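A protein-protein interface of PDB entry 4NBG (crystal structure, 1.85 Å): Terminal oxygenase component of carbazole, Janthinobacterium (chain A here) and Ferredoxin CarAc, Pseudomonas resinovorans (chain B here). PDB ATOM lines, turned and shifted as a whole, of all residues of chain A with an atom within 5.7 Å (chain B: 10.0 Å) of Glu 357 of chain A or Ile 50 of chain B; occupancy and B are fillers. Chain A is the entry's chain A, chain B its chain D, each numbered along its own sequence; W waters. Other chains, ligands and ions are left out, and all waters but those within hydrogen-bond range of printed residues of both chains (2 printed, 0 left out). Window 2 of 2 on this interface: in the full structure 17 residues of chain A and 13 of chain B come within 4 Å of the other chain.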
ATOM      1  N   PRO A 206      -1.990  -3.460 -11.984  1.00  0.00           N
ATOM      2  CA  PRO A 206      -0.886  -4.058 -12.739  1.00  0.00           C
ATOM      3  C   PRO A 206       0.304  -4.537 -11.921  1.00  0.00           C
ATOM      4  O   PRO A 206       0.624  -3.974 -10.874  1.00  0.00           O
ATOM      5  CB  PRO A 206      -0.488  -2.948 -13.714  1.00  0.00           C
ATOM      6  CG  PRO A 206      -1.744  -2.143 -13.862  1.00  0.00           C
ATOM      7  CD  PRO A 206      -2.250  -2.087 -12.444  1.00  0.00           C
ATOM      8  N   ARG A 210       6.183  -2.976 -17.857  1.00  0.00           N
ATOM      9  CA  ARG A 210       5.201  -2.668 -18.889  1.00  0.00           C
ATOM     10  C   ARG A 210       5.324  -3.575 -20.104  1.00  0.00           C
ATOM     11  O   ARG A 210       4.347  -3.817 -20.808  1.00  0.00           O
ATOM     12  CB  ARG A 210       5.297  -1.197 -19.315  1.00  0.00           C
ATOM     13  CG  ARG A 210       6.388  -0.855 -20.315  1.00  0.00           C
ATOM     14  CD  ARG A 210       5.813   0.073 -21.382  1.00  0.00           C
ATOM     15  NE  ARG A 210       6.831   0.711 -22.212  1.00  0.00           N
ATOM     16  CZ  ARG A 210       7.635   1.688 -21.799  1.00  0.00           C
ATOM     17  NH1 ARG A 210       7.548   2.149 -20.556  1.00  0.00           N
ATOM     18  NH2 ARG A 210       8.522   2.215 -22.638  1.00  0.00           N
ATOM     19  N   ILE A 231      -2.697  -8.048 -18.892  1.00  0.00           N
ATOM     20  CA  ILE A 231      -2.725  -7.343 -17.614  1.00  0.00           C
ATOM     21  C   ILE A 231      -3.015  -8.286 -16.444  1.00  0.00           C
ATOM     22  O   ILE A 231      -2.586  -8.035 -15.319  1.00  0.00           O
ATOM     23  CB  ILE A 231      -3.761  -6.183 -17.636  1.00  0.00           C
ATOM     24  CG1 ILE A 231      -3.485  -5.216 -16.483  1.00  0.00           C
ATOM     25  CG2 ILE A 231      -5.181  -6.736 -17.536  1.00  0.00           C
ATOM     26  CD1 ILE A 231      -4.295  -3.920 -16.546  1.00  0.00           C
ATOM     27  N   LEU A 355      -3.676   9.383 -20.090  1.00  0.00           N
ATOM     28  CA  LEU A 355      -3.680   7.930 -19.945  1.00  0.00           C
ATOM     29  C   LEU A 355      -3.152   7.430 -18.602  1.00  0.00           C
ATOM     30  O   LEU A 355      -2.431   8.141 -17.909  1.00  0.00           O
ATOM     31  CB  LEU A 355      -2.841   7.306 -21.069  1.00  0.00           C
ATOM     32  CG  LEU A 355      -3.156   7.810 -22.483  1.00  0.00           C
ATOM     33  CD1 LEU A 355      -2.255   7.117 -23.489  1.00  0.00           C
ATOM     34  CD2 LEU A 355      -4.614   7.547 -22.807  1.00  0.00           C
ATOM     35  N   PHE A 356      -3.555   6.219 -18.220  1.00  0.00           N
ATOM     36  CA  PHE A 356      -3.040   5.629 -16.998  1.00  0.00           C
ATOM     37  C   PHE A 356      -2.557   4.212 -17.306  1.00  0.00           C
ATOM     38  O   PHE A 356      -2.632   3.770 -18.455  1.00  0.00           O
ATOM     39  CB  PHE A 356      -4.040   5.751 -15.811  1.00  0.00           C
ATOM     40  CG  PHE A 356      -5.198   4.788 -15.816  1.00  0.00           C
ATOM     41  CD1 PHE A 356      -5.862   4.436 -16.982  1.00  0.00           C
ATOM     42  CD2 PHE A 356      -5.701   4.324 -14.594  1.00  0.00           C
ATOM     43  CE1 PHE A 356      -7.014   3.642 -16.936  1.00  0.00           C
ATOM     44  CE2 PHE A 356      -6.852   3.532 -14.535  1.00  0.00           C
ATOM     45  CZ  PHE A 356      -7.510   3.191 -15.708  1.00  0.00           C
ATOM     46  N   GLU A 357      -2.030   3.520 -16.305  1.00  0.00           N
ATOM     47  CA  GLU A 357      -1.427   2.203 -16.502  1.00  0.00           C
ATOM     48  C   GLU A 357      -2.042   1.187 -17.463  1.00  0.00           C
ATOM     49  O   GLU A 357      -1.353   0.699 -18.359  1.00  0.00           O
ATOM     50  CB  GLU A 357      -1.188   1.536 -15.141  1.00  0.00           C
ATOM     51  CG  GLU A 357      -0.138   2.248 -14.274  1.00  0.00           C
ATOM     52  CD  GLU A 357      -0.691   3.450 -13.518  1.00  0.00           C
ATOM     53  OE1 GLU A 357      -1.916   3.676 -13.563  1.00  0.00           O
ATOM     54  OE2 GLU A 357       0.104   4.166 -12.867  1.00  0.00           O
ATOM     55  N   SER A 358      -3.314   0.850 -17.292  1.00  0.00           N
ATOM     56  CA  SER A 358      -3.923  -0.142 -18.172  1.00  0.00           C
ATOM     57  C   SER A 358      -3.948   0.267 -19.641  1.00  0.00           C
ATOM     58  O   SER A 358      -4.143  -0.578 -20.513  1.00  0.00           O
ATOM     59  CB  SER A 358      -5.342  -0.486 -17.703  1.00  0.00           C
ATOM     60  OG  SER A 358      -6.148   0.671 -17.617  1.00  0.00           O
ATOM     61  N   ASP A 359      -3.749   1.551 -19.920  1.00  0.00           N
ATOM     62  CA  ASP A 359      -3.747   2.015 -21.304  1.00  0.00           C
ATOM     63  C   ASP A 359      -2.506   1.548 -22.069  1.00  0.00           C
ATOM     64  O   ASP A 359      -2.349   1.845 -23.257  1.00  0.00           O
ATOM     65  CB  ASP A 359      -3.876   3.542 -21.363  1.00  0.00           C
ATOM     66  CG  ASP A 359      -5.241   4.023 -20.902  1.00  0.00           C
ATOM     67  OD1 ASP A 359      -6.250   3.371 -21.248  1.00  0.00           O
ATOM     68  OD2 ASP A 359      -5.315   5.055 -20.207  1.00  0.00           O
ATOM     69  N   GLU A 360      -1.625   0.812 -21.394  1.00  0.00           N
ATOM     70  CA  GLU A 360      -0.441   0.277 -22.065  1.00  0.00           C
ATOM     71  C   GLU A 360      -0.943  -0.612 -23.204  1.00  0.00           C
ATOM     72  O   GLU A 360      -0.298  -0.727 -24.243  1.00  0.00           O
ATOM     73  CB  GLU A 360       0.409  -0.568 -21.109  1.00  0.00           C
ATOM     74  CG  GLU A 360       1.233   0.219 -20.092  1.00  0.00           C
ATOM     75  CD  GLU A 360       2.350   1.039 -20.728  1.00  0.00           C
ATOM     76  OE1 GLU A 360       2.579   0.908 -21.953  1.00  0.00           O
ATOM     77  OE2 GLU A 360       3.007   1.815 -19.995  1.00  0.00           O
ATOM     78  N   ALA A 361      -2.101  -1.236 -23.003  1.00  0.00           N
ATOM     79  CA  ALA A 361      -2.679  -2.111 -24.025  1.00  0.00           C
ATOM     80  C   ALA A 361      -3.057  -1.295 -25.266  1.00  0.00           C
ATOM     81  O   ALA A 361      -2.761  -1.683 -26.396  1.00  0.00           O
ATOM     82  CB  ALA A 361      -3.915  -2.828 -23.468  1.00  0.00           C
ATOM     83  N   VAL A 363      -1.899   1.672 -26.108  1.00  0.00           N
ATOM     84  CA  VAL A 363      -0.676   2.207 -26.696  1.00  0.00           C
ATOM     85  C   VAL A 363       0.006   1.166 -27.595  1.00  0.00           C
ATOM     86  O   VAL A 363       0.482   1.500 -28.682  1.00  0.00           O
ATOM     87  CB  VAL A 363       0.310   2.673 -25.588  1.00  0.00           C
ATOM     88  CG1 VAL A 363       1.686   2.948 -26.182  1.00  0.00           C
ATOM     89  CG2 VAL A 363      -0.226   3.934 -24.924  1.00  0.00           C
ATOM     90  N   ARG B  21      17.971   6.162 -19.626  1.00  0.00           N
ATOM     91  CA  ARG B  21      16.988   5.656 -18.680  1.00  0.00           C
ATOM     92  C   ARG B  21      17.667   4.871 -17.569  1.00  0.00           C
ATOM     93  O   ARG B  21      18.571   4.075 -17.820  1.00  0.00           O
ATOM     94  CB  ARG B  21      15.968   4.763 -19.389  1.00  0.00           C
ATOM     95  CG  ARG B  21      15.017   4.055 -18.435  1.00  0.00           C
ATOM     96  CD  ARG B  21      13.821   3.463 -19.156  1.00  0.00           C
ATOM     97  NE  ARG B  21      12.977   2.693 -18.245  1.00  0.00           N
ATOM     98  CZ  ARG B  21      11.722   2.340 -18.501  1.00  0.00           C
ATOM     99  NH1 ARG B  21      11.151   2.692 -19.646  1.00  0.00           N
ATOM    100  NH2 ARG B  21      11.035   1.633 -17.613  1.00  0.00           N
ATOM    101  N   ALA B  28       9.963   3.296  -9.445  1.00  0.00           N
ATOM    102  CA  ALA B  28       9.725   3.886 -10.757  1.00  0.00           C
ATOM    103  C   ALA B  28      11.047   4.292 -11.407  1.00  0.00           C
ATOM    104  O   ALA B  28      12.004   4.644 -10.717  1.00  0.00           O
ATOM    105  CB  ALA B  28       8.814   5.099 -10.621  1.00  0.00           C
ATOM    106  N   PRO B  29      11.117   4.240 -12.746  1.00  0.00           N
ATOM    107  CA  PRO B  29      12.336   4.605 -13.476  1.00  0.00           C
ATOM    108  C   PRO B  29      12.625   6.103 -13.508  1.00  0.00           C
ATOM    109  O   PRO B  29      11.724   6.928 -13.361  1.00  0.00           O
ATOM    110  CB  PRO B  29      12.077   4.042 -14.871  1.00  0.00           C
ATOM    111  CG  PRO B  29      10.596   4.219 -15.015  1.00  0.00           C
ATOM    112  CD  PRO B  29      10.083   3.743 -13.671  1.00  0.00           C
ATOM    113  N   GLU B  43      11.907  12.071 -13.016  1.00  0.00           N
ATOM    114  CA  GLU B  43      11.194  10.806 -13.153  1.00  0.00           C
ATOM    115  C   GLU B  43      11.251  10.530 -14.651  1.00  0.00           C
ATOM    116  O   GLU B  43      11.336  11.467 -15.443  1.00  0.00           O
ATOM    117  CB  GLU B  43       9.721  10.953 -12.780  1.00  0.00           C
ATOM    118  CG  GLU B  43       9.411  11.822 -11.591  1.00  0.00           C
ATOM    119  CD  GLU B  43       7.914  12.022 -11.434  1.00  0.00           C
ATOM    120  OE1 GLU B  43       7.194  11.010 -11.300  1.00  0.00           O
ATOM    121  OE2 GLU B  43       7.457  13.185 -11.452  1.00  0.00           O
ATOM    122  N   ASP B  44      11.199   9.264 -15.047  1.00  0.00           N
ATOM    123  CA  ASP B  44      11.217   8.939 -16.469  1.00  0.00           C
ATOM    124  C   ASP B  44       9.807   9.043 -17.050  1.00  0.00           C
ATOM    125  O   ASP B  44       9.624   9.406 -18.212  1.00  0.00           O
ATOM    126  CB  ASP B  44      11.741   7.522 -16.699  1.00  0.00           C
ATOM    127  CG  ASP B  44      11.753   7.142 -18.168  1.00  0.00           C
ATOM    128  OD1 ASP B  44      12.424   7.842 -18.953  1.00  0.00           O
ATOM    129  OD2 ASP B  44      11.088   6.150 -18.541  1.00  0.00           O
ATOM    130  N   THR B  45       8.812   8.726 -16.231  1.00  0.00           N
ATOM    131  CA  THR B  45       7.424   8.757 -16.678  1.00  0.00           C
ATOM    132  C   THR B  45       6.858  10.167 -16.803  1.00  0.00           C
ATOM    133  O   THR B  45       6.923  10.961 -15.863  1.00  0.00           O
ATOM    134  CB  THR B  45       6.531   7.952 -15.723  1.00  0.00           C
ATOM    135  OG1 THR B  45       7.122   6.666 -15.493  1.00  0.00           O
ATOM    136  CG2 THR B  45       5.140   7.765 -16.327  1.00  0.00           C
ATOM    137  N   CYS B  46       6.305  10.476 -17.972  1.00  0.00           N
ATOM    138  CA  CYS B  46       5.710  11.785 -18.214  1.00  0.00           C
ATOM    139  C   CYS B  46       4.529  11.945 -17.261  1.00  0.00           C
ATOM    140  O   CYS B  46       3.737  11.019 -17.099  1.00  0.00           O
ATOM    141  CB  CYS B  46       5.223  11.886 -19.661  1.00  0.00           C
ATOM    142  SG  CYS B  46       4.529  13.494 -20.090  1.00  0.00           S
ATOM    143  N   THR B  47       4.412  13.115 -16.640  1.00  0.00           N
ATOM    144  CA  THR B  47       3.331  13.373 -15.694  1.00  0.00           C
ATOM    145  C   THR B  47       1.957  13.485 -16.358  1.00  0.00           C
ATOM    146  O   THR B  47       0.926  13.478 -15.679  1.00  0.00           O
ATOM    147  CB  THR B  47       3.592  14.664 -14.887  1.00  0.00           C
ATOM    148  OG1 THR B  47       3.610  15.789 -15.771  1.00  0.00           O
ATOM    149  CG2 THR B  47       4.933  14.584 -14.171  1.00  0.00           C
ATOM    150  N   HIS B  48       1.945  13.580 -17.684  1.00  0.00           N
ATOM    151  CA  HIS B  48       0.694  13.695 -18.430  1.00  0.00           C
ATOM    152  C   HIS B  48       0.120  12.333 -18.832  1.00  0.00           C
ATOM    153  O   HIS B  48      -1.000  12.247 -19.339  1.00  0.00           O
ATOM    154  CB  HIS B  48       0.917  14.560 -19.680  1.00  0.00           C
ATOM    155  CG  HIS B  48      -0.295  14.698 -20.551  1.00  0.00           C
ATOM    156  ND1 HIS B  48      -0.431  14.032 -21.750  1.00  0.00           N
ATOM    157  CD2 HIS B  48      -1.427  15.428 -20.396  1.00  0.00           C
ATOM    158  CE1 HIS B  48      -1.592  14.347 -22.299  1.00  0.00           C
ATOM    159  NE2 HIS B  48      -2.216  15.193 -21.497  1.00  0.00           N
ATOM    160  N   GLY B  49       0.881  11.269 -18.606  1.00  0.00           N
ATOM    161  CA  GLY B  49       0.399   9.950 -18.974  1.00  0.00           C
ATOM    162  C   GLY B  49       1.258   8.802 -18.487  1.00  0.00           C
ATOM    163  O   GLY B  49       1.557   8.701 -17.299  1.00  0.00           O
ATOM    164  N   ILE B  50       1.649   7.930 -19.410  1.00  0.00           N
ATOM    165  CA  ILE B  50       2.471   6.776 -19.072  1.00  0.00           C
ATOM    166  C   ILE B  50       3.679   6.642 -20.000  1.00  0.00           C
ATOM    167  O   ILE B  50       4.304   5.579 -20.074  1.00  0.00           O
ATOM    168  CB  ILE B  50       1.642   5.472 -19.136  1.00  0.00           C
ATOM    169  CG1 ILE B  50       1.017   5.306 -20.523  1.00  0.00           C
ATOM    170  CG2 ILE B  50       0.564   5.499 -18.063  1.00  0.00           C
ATOM    171  CD1 ILE B  50       0.226   4.016 -20.692  1.00  0.00           C
ATOM    172  N   ALA B  51       4.010   7.723 -20.698  1.00  0.00           N
ATOM    173  CA  ALA B  51       5.142   7.719 -21.622  1.00  0.00           C
ATOM    174  C   ALA B  51       6.489   7.757 -20.910  1.00  0.00           C
ATOM    175  O   ALA B  51       6.602   8.266 -19.792  1.00  0.00           O
ATOM    176  CB  ALA B  51       5.040   8.907 -22.563  1.00  0.00           C
ATOM    177  N   SER B  52       7.506   7.219 -21.576  1.00  0.00           N
ATOM    178  CA  SER B  52       8.866   7.211 -21.050  1.00  0.00           C
ATOM    179  C   SER B  52       9.606   8.380 -21.696  1.00  0.00           C
ATOM    180  O   SER B  52       9.872   8.363 -22.895  1.00  0.00           O
ATOM    181  CB  SER B  52       9.566   5.896 -21.403  1.00  0.00           C
ATOM    182  OG  SER B  52      10.950   5.952 -21.088  1.00  0.00           O
ATOM    183  N   LEU B  53       9.930   9.394 -20.900  1.00  0.00           N
ATOM    184  CA  LEU B  53      10.623  10.575 -21.406  1.00  0.00           C
ATOM    185  C   LEU B  53      11.998  10.265 -21.996  1.00  0.00           C
ATOM    186  O   LEU B  53      12.496  11.009 -22.839  1.00  0.00           O
ATOM    187  CB  LEU B  53      10.758  11.625 -20.294  1.00  0.00           C
ATOM    188  CG  LEU B  53       9.448  12.268 -19.822  1.00  0.00           C
ATOM    189  CD1 LEU B  53       9.714  13.140 -18.602  1.00  0.00           C
ATOM    190  CD2 LEU B  53       8.839  13.095 -20.954  1.00  0.00           C
ATOM    191  N   SER B  54      12.607   9.167 -21.562  1.00  0.00           N
ATOM    192  CA  SER B  54      13.920   8.796 -22.079  1.00  0.00           C
ATOM    193  C   SER B  54      13.814   8.362 -23.542  1.00  0.00           C
ATOM    194  O   SER B  54      14.823   8.176 -24.223  1.00  0.00           O
ATOM    195  CB  SER B  54      14.537   7.684 -21.218  1.00  0.00           C
ATOM    196  OG  SER B  54      13.688   6.556 -21.135  1.00  0.00           O
ATOM    197  N   GLU B  55      12.583   8.211 -24.024  1.00  0.00           N
ATOM    198  CA  GLU B  55      12.356   7.830 -25.411  1.00  0.00           C
ATOM    199  C   GLU B  55      11.972   9.075 -26.202  1.00  0.00           C
ATOM    200  O   GLU B  55      11.638   8.996 -27.385  1.00  0.00           O
ATOM    201  CB  GLU B  55      11.246   6.778 -25.504  1.00  0.00           C
ATOM    202  CG  GLU B  55      11.685   5.389 -25.059  1.00  0.00           C
ATOM    203  CD  GLU B  55      10.548   4.381 -25.052  1.00  0.00           C
ATOM    204  OE1 GLU B  55       9.736   4.385 -26.000  1.00  0.00           O
ATOM    205  OE2 GLU B  55      10.476   3.573 -24.103  1.00  0.00           O
ATOM    206  N   CYS B  65       8.099  14.978 -24.713  1.00  0.00           N
ATOM    207  CA  CYS B  65       7.482  13.662 -24.581  1.00  0.00           C
ATOM    208  C   CYS B  65       7.092  13.106 -25.950  1.00  0.00           C
ATOM    209  O   CYS B  65       6.509  13.812 -26.766  1.00  0.00           O
ATOM    210  CB  CYS B  65       6.242  13.756 -23.693  1.00  0.00           C
ATOM    211  SG  CYS B  65       5.398  12.188 -23.497  1.00  0.00           S
ATOM    212  N   PRO B  66       7.393  11.822 -26.208  1.00  0.00           N
ATOM    213  CA  PRO B  66       7.076  11.180 -27.487  1.00  0.00           C
ATOM    214  C   PRO B  66       5.597  10.886 -27.734  1.00  0.00           C
ATOM    215  O   PRO B  66       5.184  10.674 -28.874  1.00  0.00           O
ATOM    216  CB  PRO B  66       7.922   9.911 -27.446  1.00  0.00           C
ATOM    217  CG  PRO B  66       7.888   9.553 -26.001  1.00  0.00           C
ATOM    218  CD  PRO B  66       8.111  10.887 -25.322  1.00  0.00           C
ATOM    219  N   PHE B  67       4.800  10.880 -26.670  1.00  0.00           N
ATOM    220  CA  PHE B  67       3.376  10.594 -26.793  1.00  0.00           C
ATOM    221  C   PHE B  67       2.559  11.727 -27.399  1.00  0.00           C
ATOM    222  O   PHE B  67       1.943  11.558 -28.454  1.00  0.00           O
ATOM    223  CB  PHE B  67       2.786  10.240 -25.423  1.00  0.00           C
ATOM    224  CG  PHE B  67       2.846   8.772 -25.088  1.00  0.00           C
ATOM    225  CD1 PHE B  67       3.850   7.958 -25.600  1.00  0.00           C
ATOM    226  CD2 PHE B  67       1.916   8.216 -24.215  1.00  0.00           C
ATOM    227  CE1 PHE B  67       3.930   6.607 -25.244  1.00  0.00           C
ATOM    228  CE2 PHE B  67       1.987   6.870 -23.852  1.00  0.00           C
ATOM    229  CZ  PHE B  67       2.996   6.066 -24.367  1.00  0.00           C
ATOM    230  N   HIS B  68       2.553  12.880 -26.735  1.00  0.00           N
ATOM    231  CA  HIS B  68       1.758  14.004 -27.214  1.00  0.00           C
ATOM    232  C   HIS B  68       2.509  15.307 -27.465  1.00  0.00           C
ATOM    233  O   HIS B  68       1.899  16.317 -27.803  1.00  0.00           O
ATOM    234  CB  HIS B  68       0.607  14.263 -26.240  1.00  0.00           C
ATOM    235  CG  HIS B  68      -0.133  13.026 -25.841  1.00  0.00           C
ATOM    236  ND1 HIS B  68      -0.042  12.479 -24.579  1.00  0.00           N
ATOM    237  CD2 HIS B  68      -0.963  12.216 -26.544  1.00  0.00           C
ATOM    238  CE1 HIS B  68      -0.786  11.389 -24.521  1.00  0.00           C
ATOM    239  NE2 HIS B  68      -1.355  11.206 -25.700  1.00  0.00           N
ATOM    240  N   PHE B  72       9.110  19.374 -20.691  1.00  0.00           N
ATOM    241  CA  PHE B  72       9.527  19.865 -19.380  1.00  0.00           C
ATOM    242  C   PHE B  72      10.964  20.359 -19.436  1.00  0.00           C
ATOM    243  O   PHE B  72      11.746  19.938 -20.291  1.00  0.00           O
ATOM    244  CB  PHE B  72       9.497  18.759 -18.319  1.00  0.00           C
ATOM    245  CG  PHE B  72       8.193  18.037 -18.209  1.00  0.00           C
ATOM    246  CD1 PHE B  72       7.881  16.997 -19.081  1.00  0.00           C
ATOM    247  CD2 PHE B  72       7.282  18.375 -17.214  1.00  0.00           C
ATOM    248  CE1 PHE B  72       6.680  16.300 -18.957  1.00  0.00           C
ATOM    249  CE2 PHE B  72       6.080  17.688 -17.084  1.00  0.00           C
ATOM    250  CZ  PHE B  72       5.778  16.649 -17.956  1.00  0.00           C
ATOM    251  N   CYS B  84       1.248  19.127 -20.998  1.00  0.00           N
ATOM    252  CA  CYS B  84       1.754  18.934 -19.639  1.00  0.00           C
ATOM    253  C   CYS B  84       1.467  20.110 -18.706  1.00  0.00           C
ATOM    254  O   CYS B  84       1.570  21.269 -19.107  1.00  0.00           O
ATOM    255  CB  CYS B  84       3.257  18.664 -19.678  1.00  0.00           C
ATOM    256  SG  CYS B  84       3.676  17.150 -20.566  1.00  0.00           S
HETATM  257  O   HOH W   1      -1.729  10.883 -21.586  1.00  0.00           O
HETATM  258  O   HOH W   2       3.952   3.323 -22.652  1.00  0.00           O
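NH2 of Arg 210 of chain A is in salt-bridge range of OE2 of Glu 55 of chain B, at 2.8 Å.
The backbone NH (N) of Phe 356 of chain A lies within hydrogen-bond range of the side-chain carboxylate (OD2) of Asp 359 of chain A, at 2.9 Å. The side-chain carboxylate (OD2) of Asp 44 of chain B lies within salt-bridge range of the guanidinium group (NH1) of Arg 21 of chain B, at 3.6 Å. SG of Cys 46 of chain B lies close to N of His 48 of chain B (3.5 Å). The side-chain sulfur (SG) of Cys 65 of chain B sits close to the backbone NH (N) of Phe 67 of chain B (3.5 Å).
Among the printed residues, pairs that only touch across the chains: Phe 356 of chain A with Ile 50 of chain B (3.5 Å), Leu 355 of chain A with Gly 49 of chain B (3.5 Å), Glu 360 of chain A with Ile 50 of chain B (3.6 Å), Glu 357 of chain A with Ile 50 of chain B (3.7 Å), Arg 210 of chain A with Arg 21 of chain B (3.8 Å), Val 363 of chain A with Phe 67 of chain B (3.8 Å), Asp 359 of chain A with Ile 50 of chain B (3.9 Å), Leu 355 of chain A with His 48 of chain B (3.99 Å) and Leu 355 of chain A with Ile 50 of chain B (3.997 Å).
Phe 356 of chain A touches just one residue of chain B: Ile 50 (3.5 Å). Glu 357 of chain A touches just one residue of chain B: Ile 50 (3.7 Å). Ser 358 of chain A touches none of the printed residues of chain B. Of the printed residues of chain B, Asp 359 of chain A touches Ile 50 (3.9 Å). Of chain B, only Ile 50 comes within 4 Å of Glu 360 of chain A. Of the printed residues of chain A, Gly 49 of chain B touches Leu 355 (3.5 Å). Of the printed residues of chain A, Ile 50 of chain B touches Leu 355, Phe 356, Glu 357, Asp 359 and Glu 360. Printed residues of chain A within 4 Å of Phe 67 of chain B: Val 363. The nearest printed residue of chain A that does not touch Ile 50 of chain B is Val 363 of chain A (4.3 Å).
Hydrophobic or aromatic side chains of chain B within 4 Å of the printed part of chain A: Ile 50 and Phe 67.
Water W1 bridges the backbone carbonyl oxygen of His 48 of chain B (2.7 Å) and the backbone NH of Leu 355 of chain A (2.9 Å). Water W2 bridges OE1 of Glu 360 of chain A (2.9 Å) and O of Ile 50 of chain B (3.4 Å).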
